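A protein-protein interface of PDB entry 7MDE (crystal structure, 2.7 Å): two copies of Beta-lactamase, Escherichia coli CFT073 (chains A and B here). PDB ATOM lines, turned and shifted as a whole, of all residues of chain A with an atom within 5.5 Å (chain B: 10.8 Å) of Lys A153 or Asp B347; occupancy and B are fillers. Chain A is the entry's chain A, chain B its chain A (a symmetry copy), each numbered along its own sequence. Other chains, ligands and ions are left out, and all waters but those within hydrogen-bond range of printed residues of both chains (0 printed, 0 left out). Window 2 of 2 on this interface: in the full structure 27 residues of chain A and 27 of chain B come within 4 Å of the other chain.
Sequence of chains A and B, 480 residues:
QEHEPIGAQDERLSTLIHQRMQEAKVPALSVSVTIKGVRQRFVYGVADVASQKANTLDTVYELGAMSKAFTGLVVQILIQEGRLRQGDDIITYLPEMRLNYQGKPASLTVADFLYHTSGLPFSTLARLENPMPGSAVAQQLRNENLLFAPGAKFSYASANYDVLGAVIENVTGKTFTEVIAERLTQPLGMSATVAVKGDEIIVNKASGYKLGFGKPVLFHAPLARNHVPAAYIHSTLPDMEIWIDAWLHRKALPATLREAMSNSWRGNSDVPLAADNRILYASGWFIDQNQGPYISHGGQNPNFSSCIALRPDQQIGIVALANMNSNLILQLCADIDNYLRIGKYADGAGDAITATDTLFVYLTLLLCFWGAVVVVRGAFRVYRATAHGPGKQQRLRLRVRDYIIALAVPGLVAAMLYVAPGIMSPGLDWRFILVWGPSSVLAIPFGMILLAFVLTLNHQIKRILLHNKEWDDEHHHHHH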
ATOM      1  N   HIS A 116       1.287 -19.413   8.217  1.00  0.00           N
ATOM      2  CA  HIS A 116      -0.116 -19.818   8.389  1.00  0.00           C
ATOM      3  C   HIS A 116      -0.481 -20.092   9.859  1.00  0.00           C
ATOM      4  O   HIS A 116      -1.210 -21.039  10.165  1.00  0.00           O
ATOM      5  CB  HIS A 116      -0.443 -21.051   7.523  1.00  0.00           C
ATOM      6  CG  HIS A 116      -0.184 -20.868   6.051  1.00  0.00           C
ATOM      7  ND1 HIS A 116      -1.173 -20.508   5.160  1.00  0.00           N
ATOM      8  CD2 HIS A 116       0.942 -21.036   5.309  1.00  0.00           C
ATOM      9  CE1 HIS A 116      -0.664 -20.429   3.940  1.00  0.00           C
ATOM     10  NE2 HIS A 116       0.617 -20.747   4.002  1.00  0.00           N
ATOM     11  N   THR A 117       0.036 -19.276  10.789  1.00  0.00           N
ATOM     12  CA  THR A 117      -0.368 -19.348  12.195  1.00  0.00           C
ATOM     13  C   THR A 117      -1.267 -18.175  12.598  1.00  0.00           C
ATOM     14  O   THR A 117      -1.243 -17.731  13.753  1.00  0.00           O
ATOM     15  CB  THR A 117       0.842 -19.423  13.136  1.00  0.00           C
ATOM     16  OG1 THR A 117       1.639 -18.236  13.018  1.00  0.00           O
ATOM     17  CG2 THR A 117       1.696 -20.596  12.809  1.00  0.00           C
ATOM     18  N   SER A 118      -2.094 -17.686  11.667  1.00  0.00           N
ATOM     19  CA  SER A 118      -2.855 -16.458  11.891  1.00  0.00           C
ATOM     20  C   SER A 118      -4.229 -16.682  12.516  1.00  0.00           C
ATOM     21  O   SER A 118      -4.733 -15.802  13.224  1.00  0.00           O
ATOM     22  CB  SER A 118      -3.043 -15.712  10.569  1.00  0.00           C
ATOM     23  OG  SER A 118      -4.135 -16.234   9.823  1.00  0.00           O
ATOM     24  N   LEU A 147      -9.876 -18.163  14.296  1.00  0.00           N
ATOM     25  CA  LEU A 147     -10.209 -19.489  14.810  1.00  0.00           C
ATOM     26  C   LEU A 147      -9.432 -19.872  16.074  1.00  0.00           C
ATOM     27  O   LEU A 147      -9.824 -20.822  16.751  1.00  0.00           O
ATOM     28  CB  LEU A 147      -9.953 -20.542  13.715  1.00  0.00           C
ATOM     29  CG  LEU A 147     -10.564 -20.285  12.328  1.00  0.00           C
ATOM     30  CD1 LEU A 147      -9.939 -21.178  11.257  1.00  0.00           C
ATOM     31  CD2 LEU A 147     -12.097 -20.429  12.346  1.00  0.00           C
ATOM     32  N   PHE A 148      -8.353 -19.172  16.403  1.00  0.00           N
ATOM     33  CA  PHE A 148      -7.520 -19.490  17.555  1.00  0.00           C
ATOM     34  C   PHE A 148      -6.586 -18.311  17.787  1.00  0.00           C
ATOM     35  O   PHE A 148      -6.532 -17.374  16.988  1.00  0.00           O
ATOM     36  CB  PHE A 148      -6.727 -20.785  17.363  1.00  0.00           C
ATOM     37  CG  PHE A 148      -6.069 -20.905  16.029  1.00  0.00           C
ATOM     38  CD1 PHE A 148      -4.863 -20.268  15.769  1.00  0.00           C
ATOM     39  CD2 PHE A 148      -6.651 -21.660  15.019  1.00  0.00           C
ATOM     40  CE1 PHE A 148      -4.250 -20.362  14.503  1.00  0.00           C
ATOM     41  CE2 PHE A 148      -6.039 -21.763  13.766  1.00  0.00           C
ATOM     42  CZ  PHE A 148      -4.838 -21.118  13.514  1.00  0.00           C
ATOM     43  N   ALA A 149      -5.867 -18.346  18.902  1.00  0.00           N
ATOM     44  CA  ALA A 149      -4.905 -17.289  19.154  1.00  0.00           C
ATOM     45  C   ALA A 149      -3.831 -17.311  18.072  1.00  0.00           C
ATOM     46  O   ALA A 149      -3.462 -18.388  17.593  1.00  0.00           O
ATOM     47  CB  ALA A 149      -4.266 -17.455  20.525  1.00  0.00           C
ATOM     48  N   GLY A 151      -0.377 -17.658  16.301  1.00  0.00           N
ATOM     49  CA  GLY A 151       0.783 -18.443  16.665  1.00  0.00           C
ATOM     50  C   GLY A 151       0.500 -19.772  17.338  1.00  0.00           C
ATOM     51  O   GLY A 151       1.454 -20.500  17.641  1.00  0.00           O
ATOM     52  N   ALA A 152      -0.773 -20.127  17.572  1.00  0.00           N
ATOM     53  CA  ALA A 152      -1.101 -21.282  18.403  1.00  0.00           C
ATOM     54  C   ALA A 152      -1.172 -22.583  17.626  1.00  0.00           C
ATOM     55  O   ALA A 152      -1.126 -23.653  18.240  1.00  0.00           O
ATOM     56  CB  ALA A 152      -2.439 -21.075  19.123  1.00  0.00           C
ATOM     57  N   LYS A 153      -1.272 -22.522  16.301  1.00  0.00           N
ATOM     58  CA  LYS A 153      -1.609 -23.686  15.492  1.00  0.00           C
ATOM     59  C   LYS A 153      -1.269 -23.361  14.041  1.00  0.00           C
ATOM     60  O   LYS A 153      -1.363 -22.196  13.619  1.00  0.00           O
ATOM     61  CB  LYS A 153      -3.101 -24.037  15.666  1.00  0.00           C
ATOM     62  CG  LYS A 153      -3.627 -25.254  14.925  1.00  0.00           C
ATOM     63  CD  LYS A 153      -5.168 -25.261  14.941  1.00  0.00           C
ATOM     64  CE  LYS A 153      -5.741 -24.996  16.347  1.00  0.00           C
ATOM     65  NZ  LYS A 153      -7.246 -24.963  16.412  1.00  0.00           N
ATOM     66  N   PHE A 154      -0.820 -24.387  13.302  1.00  0.00           N
ATOM     67  CA  PHE A 154      -0.707 -24.296  11.852  1.00  0.00           C
ATOM     68  C   PHE A 154      -2.055 -24.591  11.225  1.00  0.00           C
ATOM     69  O   PHE A 154      -2.667 -25.606  11.537  1.00  0.00           O
ATOM     70  CB  PHE A 154       0.317 -25.278  11.301  1.00  0.00           C
ATOM     71  CG  PHE A 154       0.310 -25.349   9.794  1.00  0.00           C
ATOM     72  CD1 PHE A 154       1.036 -24.422   9.036  1.00  0.00           C
ATOM     73  CD2 PHE A 154      -0.454 -26.311   9.126  1.00  0.00           C
ATOM     74  CE1 PHE A 154       1.021 -24.468   7.623  1.00  0.00           C
ATOM     75  CE2 PHE A 154      -0.493 -26.360   7.724  1.00  0.00           C
ATOM     76  CZ  PHE A 154       0.254 -25.444   6.972  1.00  0.00           C
ATOM     77  N   SER A 155      -2.512 -23.704  10.346  1.00  0.00           N
ATOM     78  CA  SER A 155      -3.776 -23.887   9.627  1.00  0.00           C
ATOM     79  C   SER A 155      -3.644 -23.162   8.289  1.00  0.00           C
ATOM     80  O   SER A 155      -3.596 -21.930   8.251  1.00  0.00           O
ATOM     81  CB  SER A 155      -4.952 -23.357  10.453  1.00  0.00           C
ATOM     82  OG  SER A 155      -6.174 -23.393   9.739  1.00  0.00           O
ATOM     83  N   VAL A 271       4.942 -24.716  16.574  1.00  0.00           N
ATOM     84  CA  VAL A 271       3.532 -25.091  16.471  1.00  0.00           C
ATOM     85  C   VAL A 271       3.383 -26.534  16.931  1.00  0.00           C
ATOM     86  O   VAL A 271       4.361 -27.294  16.989  1.00  0.00           O
ATOM     87  CB  VAL A 271       2.996 -24.930  15.033  1.00  0.00           C
ATOM     88  CG1 VAL A 271       2.184 -23.659  14.895  1.00  0.00           C
ATOM     89  CG2 VAL A 271       4.149 -24.958  14.064  1.00  0.00           C
ATOM     90  N   PRO A 272       2.169 -26.932  17.303  1.00  0.00           N
ATOM     91  CA  PRO A 272       1.940 -28.344  17.622  1.00  0.00           C
ATOM     92  C   PRO A 272       1.976 -29.187  16.361  1.00  0.00           C
ATOM     93  O   PRO A 272       1.518 -28.773  15.292  1.00  0.00           O
ATOM     94  CB  PRO A 272       0.541 -28.353  18.261  1.00  0.00           C
ATOM     95  CG  PRO A 272       0.321 -26.984  18.729  1.00  0.00           C
ATOM     96  CD  PRO A 272       1.017 -26.107  17.689  1.00  0.00           C
ATOM     97  N   LEU B  16      -3.594 -31.311  31.078  1.00  0.00           N
ATOM     98  CA  LEU B  16      -3.753 -31.857  29.737  1.00  0.00           C
ATOM     99  C   LEU B  16      -4.266 -33.286  29.788  1.00  0.00           C
ATOM    100  O   LEU B  16      -5.211 -33.642  29.074  1.00  0.00           O
ATOM    101  CB  LEU B  16      -2.420 -31.785  28.995  1.00  0.00           C
ATOM    102  CG  LEU B  16      -2.296 -32.676  27.760  1.00  0.00           C
ATOM    103  CD1 LEU B  16      -3.320 -32.313  26.696  1.00  0.00           C
ATOM    104  CD2 LEU B  16      -0.882 -32.582  27.209  1.00  0.00           C
ATOM    105  N   GLN B  19      -7.799 -33.600  31.118  1.00  0.00           N
ATOM    106  CA  GLN B  19      -8.737 -33.087  30.124  1.00  0.00           C
ATOM    107  C   GLN B  19      -8.960 -34.089  28.993  1.00  0.00           C
ATOM    108  O   GLN B  19     -10.102 -34.387  28.622  1.00  0.00           O
ATOM    109  CB  GLN B  19      -8.224 -31.759  29.568  1.00  0.00           C
ATOM    110  CG  GLN B  19      -9.234 -31.049  28.714  1.00  0.00           C
ATOM    111  CD  GLN B  19      -8.582 -30.146  27.697  1.00  0.00           C
ATOM    112  OE1 GLN B  19      -7.745 -29.309  28.041  1.00  0.00           O
ATOM    113  NE2 GLN B  19      -8.950 -30.317  26.430  1.00  0.00           N
ATOM    114  N   ARG B  20      -7.875 -34.603  28.415  1.00  0.00           N
ATOM    115  CA  ARG B  20      -7.991 -35.675  27.432  1.00  0.00           C
ATOM    116  C   ARG B  20      -8.747 -36.880  27.982  1.00  0.00           C
ATOM    117  O   ARG B  20      -9.475 -37.550  27.236  1.00  0.00           O
ATOM    118  CB  ARG B  20      -6.602 -36.096  26.971  1.00  0.00           C
ATOM    119  CG  ARG B  20      -5.950 -35.063  26.099  1.00  0.00           C
ATOM    120  CD  ARG B  20      -6.867 -34.710  24.931  1.00  0.00           C
ATOM    121  NE  ARG B  20      -6.112 -34.072  23.866  1.00  0.00           N
ATOM    122  CZ  ARG B  20      -5.995 -32.763  23.723  1.00  0.00           C
ATOM    123  NH1 ARG B  20      -6.648 -31.925  24.508  1.00  0.00           N
ATOM    124  NH2 ARG B  20      -5.200 -32.284  22.769  1.00  0.00           N
ATOM    125  N   GLU B  23     -12.482 -35.924  28.041  1.00  0.00           N
ATOM    126  CA  GLU B  23     -12.974 -35.866  26.665  1.00  0.00           C
ATOM    127  C   GLU B  23     -13.207 -37.261  26.122  1.00  0.00           C
ATOM    128  O   GLU B  23     -14.276 -37.553  25.573  1.00  0.00           O
ATOM    129  CB  GLU B  23     -11.977 -35.146  25.758  1.00  0.00           C
ATOM    130  CG  GLU B  23     -11.925 -33.644  25.850  1.00  0.00           C
ATOM    131  CD  GLU B  23     -10.819 -33.096  24.979  1.00  0.00           C
ATOM    132  OE1 GLU B  23     -11.125 -32.627  23.857  1.00  0.00           O
ATOM    133  OE2 GLU B  23      -9.639 -33.180  25.395  1.00  0.00           O
ATOM    134  N   ALA B  24     -12.192 -38.127  26.254  1.00  0.00           N
ATOM    135  CA  ALA B  24     -12.252 -39.479  25.717  1.00  0.00           C
ATOM    136  C   ALA B  24     -13.259 -40.343  26.465  1.00  0.00           C
ATOM    137  O   ALA B  24     -13.783 -41.303  25.897  1.00  0.00           O
ATOM    138  CB  ALA B  24     -10.867 -40.127  25.764  1.00  0.00           C
ATOM    139  N   ASN B 327      -9.405 -42.447  20.024  1.00  0.00           N
ATOM    140  CA  ASN B 327      -8.375 -41.709  19.296  1.00  0.00           C
ATOM    141  C   ASN B 327      -7.673 -40.693  20.199  1.00  0.00           C
ATOM    142  O   ASN B 327      -6.481 -40.410  20.013  1.00  0.00           O
ATOM    143  CB  ASN B 327      -8.986 -41.016  18.070  1.00  0.00           C
ATOM    144  CG  ASN B 327      -7.927 -40.458  17.101  1.00  0.00           C
ATOM    145  OD1 ASN B 327      -6.997 -41.167  16.695  1.00  0.00           O
ATOM    146  ND2 ASN B 327      -8.073 -39.179  16.729  1.00  0.00           N
ATOM    147  N   LEU B 328      -8.380 -40.149  21.195  1.00  0.00           N
ATOM    148  CA  LEU B 328      -7.750 -39.187  22.088  1.00  0.00           C
ATOM    149  C   LEU B 328      -6.613 -39.800  22.887  1.00  0.00           C
ATOM    150  O   LEU B 328      -5.788 -39.057  23.434  1.00  0.00           O
ATOM    151  CB  LEU B 328      -8.793 -38.568  23.016  1.00  0.00           C
ATOM    152  CG  LEU B 328      -9.701 -37.587  22.268  1.00  0.00           C
ATOM    153  CD1 LEU B 328     -11.023 -38.224  21.887  1.00  0.00           C
ATOM    154  CD2 LEU B 328      -9.931 -36.365  23.090  1.00  0.00           C
ATOM    155  N   ILE B 329      -6.538 -41.130  22.947  1.00  0.00           N
ATOM    156  CA  ILE B 329      -5.455 -41.825  23.633  1.00  0.00           C
ATOM    157  C   ILE B 329      -4.383 -42.174  22.611  1.00  0.00           C
ATOM    158  O   ILE B 329      -3.187 -42.171  22.924  1.00  0.00           O
ATOM    159  CB  ILE B 329      -5.971 -43.072  24.381  1.00  0.00           C
ATOM    160  CG1 ILE B 329      -7.022 -42.666  25.419  1.00  0.00           C
ATOM    161  CG2 ILE B 329      -4.834 -43.806  25.080  1.00  0.00           C
ATOM    162  CD1 ILE B 329      -6.574 -41.521  26.326  1.00  0.00           C
ATOM    163  N   GLN B 331      -3.571 -40.252  20.284  1.00  0.00           N
ATOM    164  CA  GLN B 331      -2.912 -38.975  20.061  1.00  0.00           C
ATOM    165  C   GLN B 331      -2.256 -38.410  21.306  1.00  0.00           C
ATOM    166  O   GLN B 331      -1.455 -37.473  21.181  1.00  0.00           O
ATOM    167  CB  GLN B 331      -3.905 -37.927  19.541  1.00  0.00           C
ATOM    168  CG  GLN B 331      -4.708 -38.369  18.355  1.00  0.00           C
ATOM    169  CD  GLN B 331      -3.853 -39.004  17.282  1.00  0.00           C
ATOM    170  OE1 GLN B 331      -2.803 -38.471  16.905  1.00  0.00           O
ATOM    171  NE2 GLN B 331      -4.289 -40.161  16.790  1.00  0.00           N
ATOM    172  N   LEU B 332      -2.591 -38.931  22.492  1.00  0.00           N
ATOM    173  CA  LEU B 332      -2.121 -38.315  23.726  1.00  0.00           C
ATOM    174  C   LEU B 332      -0.604 -38.179  23.748  1.00  0.00           C
ATOM    175  O   LEU B 332      -0.078 -37.175  24.236  1.00  0.00           O
ATOM    176  CB  LEU B 332      -2.604 -39.123  24.932  1.00  0.00           C
ATOM    177  CG  LEU B 332      -2.266 -38.520  26.297  1.00  0.00           C
ATOM    178  CD1 LEU B 332      -2.721 -37.073  26.345  1.00  0.00           C
ATOM    179  CD2 LEU B 332      -2.929 -39.310  27.415  1.00  0.00           C
ATOM    180  N   ALA B 334       1.510 -37.693  21.216  1.00  0.00           N
ATOM    181  CA  ALA B 334       1.876 -36.508  20.441  1.00  0.00           C
ATOM    182  C   ALA B 334       1.588 -35.220  21.215  1.00  0.00           C
ATOM    183  O   ALA B 334       2.367 -34.261  21.148  1.00  0.00           O
ATOM    184  CB  ALA B 334       1.142 -36.511  19.102  1.00  0.00           C
ATOM    185  N   ASP B 335       0.455 -35.172  21.931  1.00  0.00           N
ATOM    186  CA  ASP B 335       0.120 -34.008  22.754  1.00  0.00           C
ATOM    187  C   ASP B 335       1.191 -33.766  23.804  1.00  0.00           C
ATOM    188  O   ASP B 335       1.725 -32.657  23.924  1.00  0.00           O
ATOM    189  CB  ASP B 335      -1.228 -34.209  23.453  1.00  0.00           C
ATOM    190  CG  ASP B 335      -2.418 -34.107  22.516  1.00  0.00           C
ATOM    191  OD1 ASP B 335      -2.400 -33.257  21.601  1.00  0.00           O
ATOM    192  OD2 ASP B 335      -3.381 -34.886  22.711  1.00  0.00           O
ATOM    193  N   ILE B 336       1.498 -34.798  24.597  1.00  0.00           N
ATOM    194  CA  ILE B 336       2.513 -34.676  25.634  1.00  0.00           C
ATOM    195  C   ILE B 336       3.846 -34.242  25.035  1.00  0.00           C
ATOM    196  O   ILE B 336       4.550 -33.411  25.614  1.00  0.00           O
ATOM    197  CB  ILE B 336       2.642 -35.993  26.421  1.00  0.00           C
ATOM    198  CG1 ILE B 336       1.323 -36.343  27.126  1.00  0.00           C
ATOM    199  CG2 ILE B 336       3.784 -35.891  27.440  1.00  0.00           C
ATOM    200  CD1 ILE B 336       1.410 -37.597  27.985  1.00  0.00           C
ATOM    201  N   ASN B 338       4.327 -32.490  22.208  1.00  0.00           N
ATOM    202  CA  ASN B 338       4.213 -31.078  21.860  1.00  0.00           C
ATOM    203  C   ASN B 338       4.433 -30.204  23.086  1.00  0.00           C
ATOM    204  O   ASN B 338       5.138 -29.189  23.014  1.00  0.00           O
ATOM    205  CB  ASN B 338       2.852 -30.780  21.224  1.00  0.00           C
ATOM    206  CG  ASN B 338       2.807 -31.153  19.742  1.00  0.00           C
ATOM    207  OD1 ASN B 338       3.832 -31.089  19.042  1.00  0.00           O
ATOM    208  ND2 ASN B 338       1.620 -31.545  19.256  1.00  0.00           N
ATOM    209  N   ARG B 341       7.955 -30.082  24.147  1.00  0.00           N
ATOM    210  CA  ARG B 341       8.801 -29.488  23.122  1.00  0.00           C
ATOM    211  C   ARG B 341       8.675 -27.964  23.057  1.00  0.00           C
ATOM    212  O   ARG B 341       9.689 -27.259  22.967  1.00  0.00           O
ATOM    213  CB  ARG B 341       8.451 -30.112  21.764  1.00  0.00           C
ATOM    214  CG  ARG B 341       9.507 -29.982  20.668  1.00  0.00           C
ATOM    215  CD  ARG B 341       9.097 -30.778  19.403  1.00  0.00           C
ATOM    216  NE  ARG B 341       7.763 -30.433  18.918  1.00  0.00           N
ATOM    217  CZ  ARG B 341       7.472 -29.345  18.207  1.00  0.00           C
ATOM    218  NH1 ARG B 341       8.404 -28.456  17.876  1.00  0.00           N
ATOM    219  NH2 ARG B 341       6.211 -29.136  17.823  1.00  0.00           N
ATOM    220  N   ILE B 342       7.455 -27.431  23.083  1.00  0.00           N
ATOM    221  CA  ILE B 342       7.261 -26.000  22.870  1.00  0.00           C
ATOM    222  C   ILE B 342       6.257 -25.442  23.870  1.00  0.00           C
ATOM    223  O   ILE B 342       5.843 -24.281  23.769  1.00  0.00           O
ATOM    224  CB  ILE B 342       6.796 -25.713  21.430  1.00  0.00           C
ATOM    225  CG1 ILE B 342       5.512 -26.481  21.132  1.00  0.00           C
ATOM    226  CG2 ILE B 342       7.874 -26.053  20.431  1.00  0.00           C
ATOM    227  CD1 ILE B 342       4.751 -25.931  19.952  1.00  0.00           C
ATOM    228  N   GLY B 343       5.842 -26.271  24.823  1.00  0.00           N
ATOM    229  CA  GLY B 343       4.900 -25.851  25.832  1.00  0.00           C
ATOM    230  C   GLY B 343       3.497 -25.546  25.357  1.00  0.00           C
ATOM    231  O   GLY B 343       2.795 -24.789  26.032  1.00  0.00           O
ATOM    232  N   LYS B 344       3.052 -26.098  24.224  1.00  0.00           N
ATOM    233  CA  LYS B 344       1.661 -25.920  23.800  1.00  0.00           C
ATOM    234  C   LYS B 344       1.185 -27.161  23.057  1.00  0.00           C
ATOM    235  O   LYS B 344       1.987 -27.966  22.578  1.00  0.00           O
ATOM    236  CB  LYS B 344       1.447 -24.675  22.912  1.00  0.00           C
ATOM    237  CG  LYS B 344       2.695 -24.034  22.352  1.00  0.00           C
ATOM    238  CD  LYS B 344       2.312 -22.995  21.325  1.00  0.00           C
ATOM    239  CE  LYS B 344       3.491 -22.116  20.956  1.00  0.00           C
ATOM    240  NZ  LYS B 344       3.179 -21.388  19.717  1.00  0.00           N
ATOM    241  N   TYR B 345      -0.140 -27.299  22.954  1.00  0.00           N
ATOM    242  CA  TYR B 345      -0.728 -28.498  22.373  1.00  0.00           C
ATOM    243  C   TYR B 345      -2.080 -28.182  21.741  1.00  0.00           C
ATOM    244  O   TYR B 345      -2.392 -27.082  21.294  1.00  0.00           O
ATOM    245  CB  TYR B 345      -0.867 -29.617  23.422  1.00  0.00           C
ATOM    246  CG  TYR B 345      -1.628 -29.243  24.677  1.00  0.00           C
ATOM    247  CD1 TYR B 345      -3.003 -29.056  24.651  1.00  0.00           C
ATOM    248  CD2 TYR B 345      -0.974 -29.098  25.889  1.00  0.00           C
ATOM    249  CE1 TYR B 345      -3.699 -28.734  25.789  1.00  0.00           C
ATOM    250  CE2 TYR B 345      -1.660 -28.771  27.026  1.00  0.00           C
ATOM    251  CZ  TYR B 345      -3.024 -28.591  26.977  1.00  0.00           C
ATOM    252  OH  TYR B 345      -3.728 -28.251  28.123  1.00  0.00           O
ATOM    253  N   ALA B 346      -2.438 -28.977  20.733  1.00  0.00           N
ATOM    254  CA  ALA B 346      -3.630 -28.760  19.927  1.00  0.00           C
ATOM    255  C   ALA B 346      -4.879 -29.219  20.665  1.00  0.00           C
ATOM    256  O   ALA B 346      -4.819 -29.944  21.658  1.00  0.00           O
ATOM    257  CB  ALA B 346      -3.526 -29.507  18.597  1.00  0.00           C
ATOM    258  N   ASP B 347      -6.025 -28.780  20.169  1.00  0.00           N
ATOM    259  CA  ASP B 347      -7.273 -29.315  20.679  1.00  0.00           C
ATOM    260  C   ASP B 347      -7.376 -30.785  20.292  1.00  0.00           C
ATOM    261  O   ASP B 347      -6.865 -31.211  19.246  1.00  0.00           O
ATOM    262  CB  ASP B 347      -8.471 -28.524  20.142  1.00  0.00           C
ATOM    263  CG  ASP B 347      -8.056 -27.312  19.316  1.00  0.00           C
ATOM    264  OD1 ASP B 347      -7.711 -27.490  18.124  1.00  0.00           O
ATOM    265  OD2 ASP B 347      -8.077 -26.181  19.852  1.00  0.00           O
ATOM    266  N   GLY B 348      -8.015 -31.570  21.167  1.00  0.00           N
ATOM    267  CA  GLY B 348      -8.249 -32.977  20.900  1.00  0.00           C
ATOM    268  C   GLY B 348      -8.863 -33.231  19.534  1.00  0.00           C
ATOM    269  O   GLY B 348      -9.803 -32.539  19.123  1.00  0.00           O
ATOM    270  N   ALA B 349      -8.324 -34.202  18.800  1.00  0.00           N
ATOM    271  CA  ALA B 349      -8.927 -34.573  17.531  1.00  0.00           C
ATOM    272  C   ALA B 349     -10.255 -35.286  17.789  1.00  0.00           C
ATOM    273  O   ALA B 349     -10.684 -35.473  18.932  1.00  0.00           O
ATOM    274  CB  ALA B 349      -7.965 -35.436  16.720  1.00  0.00           C
ATOM    275  N   GLY B 350     -10.933 -35.678  16.715  1.00  0.00           N
ATOM    276  CA  GLY B 350     -12.178 -36.409  16.853  1.00  0.00           C
ATOM    277  C   GLY B 350     -11.951 -37.847  17.297  1.00  0.00           C
ATOM    278  O   GLY B 350     -10.840 -38.268  17.623  1.00  0.00           O
ATOM    279  N   ASP B 351     -13.041 -38.617  17.316  1.00  0.00           N
ATOM    280  CA  ASP B 351     -12.970 -40.047  17.607  1.00  0.00           C
ATOM    281  C   ASP B 351     -13.983 -40.769  16.727  1.00  0.00           C
ATOM    282  O   ASP B 351     -15.163 -40.402  16.701  1.00  0.00           O
ATOM    283  CB  ASP B 351     -13.224 -40.348  19.099  1.00  0.00           C
ATOM    284  CG  ASP B 351     -13.113 -41.839  19.434  1.00  0.00           C
ATOM    285  OD1 ASP B 351     -11.986 -42.400  19.365  1.00  0.00           O
ATOM    286  OD2 ASP B 351     -14.154 -42.450  19.774  1.00  0.00           O
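No position is printed for both chains.
Of the 8 pairs that touch across the chains among the printed residues, none has its exchanged pair printed and touching as well.
O of Gly A151 lies within hydrogen-bond range of NZ of Lys B344, at 2.8 Å.
NZ of Lys A153 is in salt-bridge range of OD1 of Asp B347 (3.1 Å).
The guanidinium group of Arg B341 lies within hydrogen-bond range of the backbone carbonyl oxygen of Val A271 (2.7 Å).
Lys A153 touches just one residue of chain B: Asp B347 (3.1 Å).
Asp B347 touches one residue of chain A.
No residue of chain B comes within 4 Å of Ala A152.
No residue of chain B comes within 4 Å of Ser A155.
Of chain B, only Asn B338 (3.5 Å), Ile B342 (3.8 Å), Tyr B345 (3.7 Å) and Ala B346 (3.9 Å) come within 4 Å of Pro A272.
Printed residues of chain A within 4 Å of Ile B342: Val A271 (3.3 Å) and Pro A272 (3.8 Å).
Of the printed residues of chain A, Asn B338 touches Pro A272 (3.5 Å).
Of the printed residues of chain A, Tyr B345 touches Pro A272.
Printed residues of chain A within 4 Å of Arg B341: Val A271 (2.7 Å).
Of the printed residues of chain A, Lys B344 touches Gly A151 (2.8 Å).
The backbone carbonyl oxygen (O) of Ala B334 is in hydrogen-bond range of the side-chain amide nitrogen (ND2) of Asn B338 (3.4 Å).
The backbone carbonyl oxygen of Ala B346 lies within hydrogen-bond range of the guanidinium group of Arg B20, at 2.6 Å.
N of Gly A151 sits at hydrogen-bond distance from O of Thr A117 (2.7 Å).
The side-chain amide oxygen (OD1) of Asn B338 sits at hydrogen-bond distance from the guanidinium group (NH2) of Arg B341 (3.3 Å).
Among the printed residues, merely in contact across the chains: Val A271 with Ile B342 (3.3 Å), Pro A272 with Asn B338 (3.5 Å), Pro A272 with Tyr B345 (3.7 Å), Pro A272 with Ile B342 (3.8 Å) and Pro A272 with Ala B346 (3.9 Å).
Of the 13 printed residues of chain A, 4 touch a printed residue of chain B.
Hydrophobic or aromatic side chains of chain A within 4 Å of the printed part of chain B: Pro A272.
Of the 25 printed residues of chain B, 7 touch a printed residue of chain A.
Printed residues of chain B that touch a printed residue of chain A: Asn B338, Arg B341, Ile B342, Lys B344, Tyr B345, Ala B346 and Asp B347.
Hydrophobic or aromatic side chains of chain B within 4 Å of the printed part of chain A: Ile B342.
Among the printed residues, 8 pairs touch across the chains.
Among the printed residues, Asp or Glu carboxylates within 4 Å of a Lys or Arg side-chain nitrogen of the other chain: Lys A153 with Asp B347 (3.1 Å).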
